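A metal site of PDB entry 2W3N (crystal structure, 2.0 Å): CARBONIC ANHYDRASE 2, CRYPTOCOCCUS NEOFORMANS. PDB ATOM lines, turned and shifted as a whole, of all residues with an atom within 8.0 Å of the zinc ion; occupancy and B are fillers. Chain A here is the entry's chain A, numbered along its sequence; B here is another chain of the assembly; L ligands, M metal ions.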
ATOM      1  N   GLY A  67      19.667   6.586  26.182  1.00  0.00           N
ATOM      2  CA  GLY A  67      20.778   5.642  26.390  1.00  0.00           C
ATOM      3  C   GLY A  67      21.011   4.758  25.202  1.00  0.00           C
ATOM      4  O   GLY A  67      20.371   4.916  24.160  1.00  0.00           O
ATOM      5  N   CYS A  68      21.938   3.823  25.354  1.00  0.00           N
ATOM      6  CA  CYS A  68      22.323   2.943  24.252  1.00  0.00           C
ATOM      7  C   CYS A  68      21.530   1.660  24.312  1.00  0.00           C
ATOM      8  O   CYS A  68      21.161   1.206  25.409  1.00  0.00           O
ATOM      9  CB  CYS A  68      23.837   2.621  24.279  1.00  0.00           C
ATOM     10  SG  CYS A  68      24.416   1.668  22.808  1.00  0.00           S
ATOM     11  N   ALA A  69      21.257   1.099  23.150  1.00  0.00           N
ATOM     12  CA  ALA A  69      20.684  -0.218  22.983  1.00  0.00           C
ATOM     13  C   ALA A  69      21.478  -1.361  23.618  1.00  0.00           C
ATOM     14  O   ALA A  69      20.908  -2.418  23.887  1.00  0.00           O
ATOM     15  CB  ALA A  69      20.530  -0.498  21.499  1.00  0.00           C
ATOM     16  N   ASP A  70      22.768  -1.174  23.824  1.00  0.00           N
ATOM     17  CA  ASP A  70      23.598  -2.227  24.414  1.00  0.00           C
ATOM     18  C   ASP A  70      22.900  -2.961  25.592  1.00  0.00           C
ATOM     19  O   ASP A  70      22.361  -2.317  26.512  1.00  0.00           O
ATOM     20  CB  ASP A  70      24.869  -1.576  24.912  1.00  0.00           C
ATOM     21  CG  ASP A  70      25.966  -2.563  25.222  1.00  0.00           C
ATOM     22  OD1 ASP A  70      25.910  -3.166  26.309  1.00  0.00           O
ATOM     23  OD2 ASP A  70      26.920  -2.678  24.422  1.00  0.00           O
ATOM     24  N   SER A  71      22.953  -4.299  25.560  1.00  0.00           N
ATOM     25  CA  SER A  71      22.246  -5.139  26.494  1.00  0.00           C
ATOM     26  C   SER A  71      22.824  -5.029  27.921  1.00  0.00           C
ATOM     27  O   SER A  71      22.150  -5.403  28.890  1.00  0.00           O
ATOM     28  CB  SER A  71      22.305  -6.589  26.012  1.00  0.00           C
ATOM     29  OG  SER A  71      23.587  -7.126  26.287  1.00  0.00           O
ATOM     30  N   ARG A  72      24.047  -4.518  28.058  1.00  0.00           N
ATOM     31  CA  ARG A  72      24.668  -4.376  29.377  1.00  0.00           C
ATOM     32  C   ARG A  72      24.240  -3.109  30.082  1.00  0.00           C
ATOM     33  O   ARG A  72      24.694  -2.818  31.191  1.00  0.00           O
ATOM     34  CB  ARG A  72      26.199  -4.387  29.248  1.00  0.00           C
ATOM     35  CG  ARG A  72      26.714  -5.746  28.694  1.00  0.00           C
ATOM     36  CD  ARG A  72      28.113  -5.614  28.183  1.00  0.00           C
ATOM     37  NE  ARG A  72      28.161  -4.792  26.982  1.00  0.00           N
ATOM     38  CZ  ARG A  72      29.286  -4.588  26.304  1.00  0.00           C
ATOM     39  NH1 ARG A  72      30.426  -5.128  26.728  1.00  0.00           N
ATOM     40  NH2 ARG A  72      29.268  -3.857  25.206  1.00  0.00           N
ATOM     41  N   VAL A  73      23.387  -2.293  29.451  1.00  0.00           N
ATOM     42  CA  VAL A  73      23.034  -1.001  30.055  1.00  0.00           C
ATOM     43  C   VAL A  73      21.515  -0.735  30.246  1.00  0.00           C
ATOM     44  O   VAL A  73      20.990   0.255  29.702  1.00  0.00           O
ATOM     45  CB  VAL A  73      23.711   0.158  29.273  1.00  0.00           C
ATOM     46  CG1 VAL A  73      23.730   1.450  30.121  1.00  0.00           C
ATOM     47  CG2 VAL A  73      25.149  -0.213  28.953  1.00  0.00           C
ATOM     48  N   ASN A  91      18.690   3.679  21.571  1.00  0.00           N
ATOM     49  CA  ASN A  91      19.013   3.383  20.185  1.00  0.00           C
ATOM     50  C   ASN A  91      20.488   3.121  20.177  1.00  0.00           C
ATOM     51  O   ASN A  91      21.116   3.179  21.239  1.00  0.00           O
ATOM     52  CB  ASN A  91      18.621   4.571  19.277  1.00  0.00           C
ATOM     53  CG  ASN A  91      19.230   5.924  19.730  1.00  0.00           C
ATOM     54  OD1 ASN A  91      20.277   5.966  20.353  1.00  0.00           O
ATOM     55  ND2 ASN A  91      18.589   7.012  19.376  1.00  0.00           N
ATOM     56  N   VAL A  92      21.073   2.824  19.027  1.00  0.00           N
ATOM     57  CA  VAL A  92      22.516   2.556  18.939  1.00  0.00           C
ATOM     58  C   VAL A  92      23.353   3.810  19.266  1.00  0.00           C
ATOM     59  O   VAL A  92      23.143   4.859  18.708  1.00  0.00           O
ATOM     60  CB  VAL A  92      22.909   1.973  17.573  1.00  0.00           C
ATOM     61  CG1 VAL A  92      24.459   1.944  17.412  1.00  0.00           C
ATOM     62  CG2 VAL A  92      22.323   0.576  17.433  1.00  0.00           C
ATOM     63  N   ALA A  93      24.282   3.690  20.215  1.00  0.00           N
ATOM     64  CA  ALA A  93      25.163   4.815  20.610  1.00  0.00           C
ATOM     65  C   ALA A  93      24.500   6.090  21.138  1.00  0.00           C
ATOM     66  O   ALA A  93      25.032   7.211  21.026  1.00  0.00           O
ATOM     67  CB  ALA A  93      26.224   5.140  19.502  1.00  0.00           C
ATOM     68  N   ASN A  94      23.323   5.926  21.715  1.00  0.00           N
ATOM     69  CA  ASN A  94      22.695   6.995  22.451  1.00  0.00           C
ATOM     70  C   ASN A  94      22.658   8.360  21.743  1.00  0.00           C
ATOM     71  O   ASN A  94      23.093   9.402  22.337  1.00  0.00           O
ATOM     72  CB  ASN A  94      23.256   7.123  23.910  1.00  0.00           C
ATOM     73  CG  ASN A  94      24.813   7.093  24.017  1.00  0.00           C
ATOM     74  OD1 ASN A  94      25.424   6.030  24.105  1.00  0.00           O
ATOM     75  ND2 ASN A  94      25.441   8.282  24.117  1.00  0.00           N
ATOM     76  N   VAL A 122      22.956   9.081  28.589  1.00  0.00           N
ATOM     77  CA  VAL A 122      23.906   8.121  29.166  1.00  0.00           C
ATOM     78  C   VAL A 122      24.657   7.274  28.123  1.00  0.00           C
ATOM     79  O   VAL A 122      24.063   6.417  27.439  1.00  0.00           O
ATOM     80  CB  VAL A 122      23.187   7.178  30.171  1.00  0.00           C
ATOM     81  CG1 VAL A 122      24.242   6.386  31.021  1.00  0.00           C
ATOM     82  CG2 VAL A 122      22.213   7.974  30.994  1.00  0.00           C
ATOM     83  N   GLY A 123      25.946   7.512  28.006  1.00  0.00           N
ATOM     84  CA  GLY A 123      26.814   6.682  27.159  1.00  0.00           C
ATOM     85  C   GLY A 123      27.415   5.586  28.016  1.00  0.00           C
ATOM     86  O   GLY A 123      27.108   5.491  29.214  1.00  0.00           O
ATOM     87  N   HIS A 124      28.251   4.737  27.441  1.00  0.00           N
ATOM     88  CA  HIS A 124      28.894   3.682  28.272  1.00  0.00           C
ATOM     89  C   HIS A 124      30.213   3.244  27.687  1.00  0.00           C
ATOM     90  O   HIS A 124      30.421   3.356  26.457  1.00  0.00           O
ATOM     91  CB  HIS A 124      27.978   2.451  28.375  1.00  0.00           C
ATOM     92  CG  HIS A 124      27.775   1.729  27.072  1.00  0.00           C
ATOM     93  ND1 HIS A 124      28.467   0.593  26.727  1.00  0.00           N
ATOM     94  CD2 HIS A 124      26.972   2.009  26.020  1.00  0.00           C
ATOM     95  CE1 HIS A 124      28.082   0.187  25.535  1.00  0.00           C
ATOM     96  NE2 HIS A 124      27.180   1.024  25.085  1.00  0.00           N
ATOM     97  N   THR A 125      31.099   2.662  28.503  1.00  0.00           N
ATOM     98  CA  THR A 125      32.390   2.226  27.942  1.00  0.00           C
ATOM     99  C   THR A 125      32.132   0.974  27.179  1.00  0.00           C
ATOM    100  O   THR A 125      31.142   0.283  27.448  1.00  0.00           O
ATOM    101  CB  THR A 125      33.440   1.957  29.047  1.00  0.00           C
ATOM    102  OG1 THR A 125      32.880   1.058  30.002  1.00  0.00           O
ATOM    103  CG2 THR A 125      33.759   3.263  29.790  1.00  0.00           C
ATOM    104  N   GLY A 126      32.937   0.681  26.170  1.00  0.00           N
ATOM    105  CA  GLY A 126      32.699  -0.541  25.399  1.00  0.00           C
ATOM    106  C   GLY A 126      31.603  -0.396  24.346  1.00  0.00           C
ATOM    107  O   GLY A 126      31.046  -1.401  23.877  1.00  0.00           O
ATOM    108  N   CYS A 127      31.299   0.823  23.956  1.00  0.00           N
ATOM    109  CA  CYS A 127      30.140   1.066  23.089  1.00  0.00           C
ATOM    110  C   CYS A 127      30.501   0.741  21.675  1.00  0.00           C
ATOM    111  O   CYS A 127      31.289   1.450  21.076  1.00  0.00           O
ATOM    112  CB  CYS A 127      29.696   2.537  23.147  1.00  0.00           C
ATOM    113  SG  CYS A 127      28.201   2.910  22.078  1.00  0.00           S
ATOM    114  N   GLY A 128      29.921  -0.340  21.135  1.00  0.00           N
ATOM    115  CA  GLY A 128      30.224  -0.756  19.767  1.00  0.00           C
ATOM    116  C   GLY A 128      29.851   0.230  18.654  1.00  0.00           C
ATOM    117  O   GLY A 128      30.485   0.262  17.603  1.00  0.00           O
ATOM    118  N   GLY A 129      28.839   1.059  18.878  1.00  0.00           N
ATOM    119  CA  GLY A 129      28.528   2.159  17.944  1.00  0.00           C
ATOM    120  C   GLY A 129      29.670   3.173  17.757  1.00  0.00           C
ATOM    121  O   GLY A 129      30.079   3.478  16.651  1.00  0.00           O
ATOM    122  N   CYS A 130      30.170   3.696  18.869  1.00  0.00           N
ATOM    123  CA  CYS A 130      31.311   4.590  18.879  1.00  0.00           C
ATOM    124  C   CYS A 130      32.592   3.886  18.428  1.00  0.00           C
ATOM    125  O   CYS A 130      33.449   4.491  17.773  1.00  0.00           O
ATOM    126  CB  CYS A 130      31.522   5.114  20.305  1.00  0.00           C
ATOM    127  SG  CYS A 130      30.197   6.209  20.822  1.00  0.00           S
ATOM    128  N   ILE A 131      32.738   2.615  18.786  1.00  0.00           N
ATOM    129  CA  ILE A 131      33.884   1.835  18.302  1.00  0.00           C
ATOM    130  C   ILE A 131      33.841   1.732  16.769  1.00  0.00           C
ATOM    131  O   ILE A 131      34.837   1.927  16.114  1.00  0.00           O
ATOM    132  CB  ILE A 131      34.001   0.468  18.983  1.00  0.00           C
ATOM    133  CG1 ILE A 131      34.544   0.658  20.407  1.00  0.00           C
ATOM    134  CG2 ILE A 131      34.912  -0.472  18.168  1.00  0.00           C
ATOM    135  CD1 ILE A 131      34.244  -0.487  21.328  1.00  0.00           C
ATOM    136  N   ILE A 173      33.510   8.430  23.167  1.00  0.00           N
ATOM    137  CA  ILE A 173      32.286   7.995  23.844  1.00  0.00           C
ATOM    138  C   ILE A 173      31.811   9.170  24.684  1.00  0.00           C
ATOM    139  O   ILE A 173      30.622   9.515  24.656  1.00  0.00           O
ATOM    140  CB  ILE A 173      32.526   6.715  24.721  1.00  0.00           C
ATOM    141  CG1 ILE A 173      32.633   5.464  23.834  1.00  0.00           C
ATOM    142  CG2 ILE A 173      31.321   6.441  25.648  1.00  0.00           C
ATOM    143  CD1 ILE A 173      33.294   4.234  24.508  1.00  0.00           C
ATOM    144  N   ASN A 176      30.683  12.049  22.587  1.00  0.00           N
ATOM    145  CA  ASN A 176      29.402  11.723  21.985  1.00  0.00           C
ATOM    146  C   ASN A 176      28.223  12.037  22.952  1.00  0.00           C
ATOM    147  O   ASN A 176      27.192  12.553  22.567  1.00  0.00           O
ATOM    148  CB  ASN A 176      29.363  10.256  21.487  1.00  0.00           C
ATOM    149  CG  ASN A 176      28.012   9.902  20.862  1.00  0.00           C
ATOM    150  OD1 ASN A 176      27.550  10.575  19.930  1.00  0.00           O
ATOM    151  ND2 ASN A 176      27.358   8.848  21.382  1.00  0.00           N
ATOM    152  N   LEU A 214      31.573   0.185  32.423  1.00  0.00           N
ATOM    153  CA  LEU A 214      31.365  -1.297  32.451  1.00  0.00           C
ATOM    154  C   LEU A 214      32.263  -1.996  33.466  1.00  0.00           C
ATOM    155  O   LEU A 214      31.860  -3.026  34.034  1.00  0.00           O
ATOM    156  CB  LEU A 214      31.524  -1.933  31.055  1.00  0.00           C
ATOM    157  CG  LEU A 214      30.253  -2.169  30.207  1.00  0.00           C
ATOM    158  CD1 LEU A 214      29.286  -1.027  30.295  1.00  0.00           C
ATOM    159  CD2 LEU A 214      30.526  -2.449  28.718  1.00  0.00           C
ATOM    160  N   GLN B  59      29.224  -8.879  25.053  1.00  0.00           N
ATOM    161  CA  GLN B  59      27.875  -9.284  25.424  1.00  0.00           C
ATOM    162  C   GLN B  59      27.369 -10.390  24.487  1.00  0.00           C
ATOM    163  O   GLN B  59      27.776 -10.464  23.334  1.00  0.00           O
ATOM    164  CB  GLN B  59      26.955  -8.078  25.331  1.00  0.00           C
ATOM    165  CG  GLN B  59      26.916  -7.490  23.903  1.00  0.00           C
ATOM    166  CD  GLN B  59      26.185  -6.211  23.795  1.00  0.00           C
ATOM    167  OE1 GLN B  59      25.014  -6.122  24.220  1.00  0.00           O
ATOM    168  NE2 GLN B  59      26.835  -5.183  23.206  1.00  0.00           N
ATOM    169  N   PHE B  87      19.154  -6.967  24.318  1.00  0.00           N
ATOM    170  CA  PHE B  87      19.540  -5.800  23.539  1.00  0.00           C
ATOM    171  C   PHE B  87      18.244  -5.024  23.286  1.00  0.00           C
ATOM    172  O   PHE B  87      17.217  -5.655  23.148  1.00  0.00           O
ATOM    173  CB  PHE B  87      20.116  -6.293  22.201  1.00  0.00           C
ATOM    174  CG  PHE B  87      21.018  -5.310  21.501  1.00  0.00           C
ATOM    175  CD1 PHE B  87      22.383  -5.236  21.837  1.00  0.00           C
ATOM    176  CD2 PHE B  87      20.545  -4.518  20.462  1.00  0.00           C
ATOM    177  CE1 PHE B  87      23.250  -4.323  21.192  1.00  0.00           C
ATOM    178  CE2 PHE B  87      21.434  -3.610  19.780  1.00  0.00           C
ATOM    179  CZ  PHE B  87      22.785  -3.539  20.160  1.00  0.00           C
ATOM    180  N   TYR B 109      22.833  -5.219  13.880  1.00  0.00           N
ATOM    181  CA  TYR B 109      23.880  -5.382  14.847  1.00  0.00           C
ATOM    182  C   TYR B 109      23.518  -6.462  15.871  1.00  0.00           C
ATOM    183  O   TYR B 109      24.353  -7.316  16.248  1.00  0.00           O
ATOM    184  CB  TYR B 109      24.137  -4.032  15.537  1.00  0.00           C
ATOM    185  CG  TYR B 109      25.388  -4.016  16.330  1.00  0.00           C
ATOM    186  CD1 TYR B 109      26.574  -3.520  15.764  1.00  0.00           C
ATOM    187  CD2 TYR B 109      25.407  -4.496  17.634  1.00  0.00           C
ATOM    188  CE1 TYR B 109      27.743  -3.485  16.503  1.00  0.00           C
ATOM    189  CE2 TYR B 109      26.568  -4.477  18.365  1.00  0.00           C
ATOM    190  CZ  TYR B 109      27.722  -3.974  17.793  1.00  0.00           C
ATOM    191  OH  TYR B 109      28.866  -3.982  18.544  1.00  0.00           O
HETATM  192  C1  LIG L   1      26.448  -0.850  21.350  1.00  0.00           C
HETATM  193  O1  LIG L   1      26.976  -0.295  22.343  1.00  0.00           O
HETATM  194  O2  LIG L   1      26.239  -2.089  21.254  1.00  0.00           O
HETATM  195  C2  LIG L   1      26.057   0.055  20.197  1.00  0.00           C
HETATM  196 ZN    ZN M   1      26.590   1.427  22.998  1.00  0.00          ZN
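The zinc ion is bound by O1 of the ligand, SG of Cys 68, NE2 of His 124 and SG of Cys 127. The zinc ion has four donor atoms within binding distance.
Asp 70 touches the zinc ion (CB to ZN, 3.96 Å). Four residues have an atom within 4 Å of the zinc ion: Cys 68, Asp 70, His 124 and Cys 127. The nearest printed residue that does not touch the zinc ion is Gly 128 (4.2 Å).
SG of Cys 68 sits close to N of Asp 70, at 3.4 Å. The side-chain carboxylate (OD2) of Asp 70 lies within hydrogen-bond range of the side-chain amide nitrogen (NE2) of Gln 59 of chain B (2.8 Å). The side-chain sulfur (SG) of Cys 68 lies close to the backbone NH (N) of Ala 93 (3.3 Å). The side-chain sulfur of Cys 127 sits close to the backbone NH of Gly 129 (3.8 Å). OD2 of Asp 70 is in salt-bridge range of NH2 of Arg 72.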
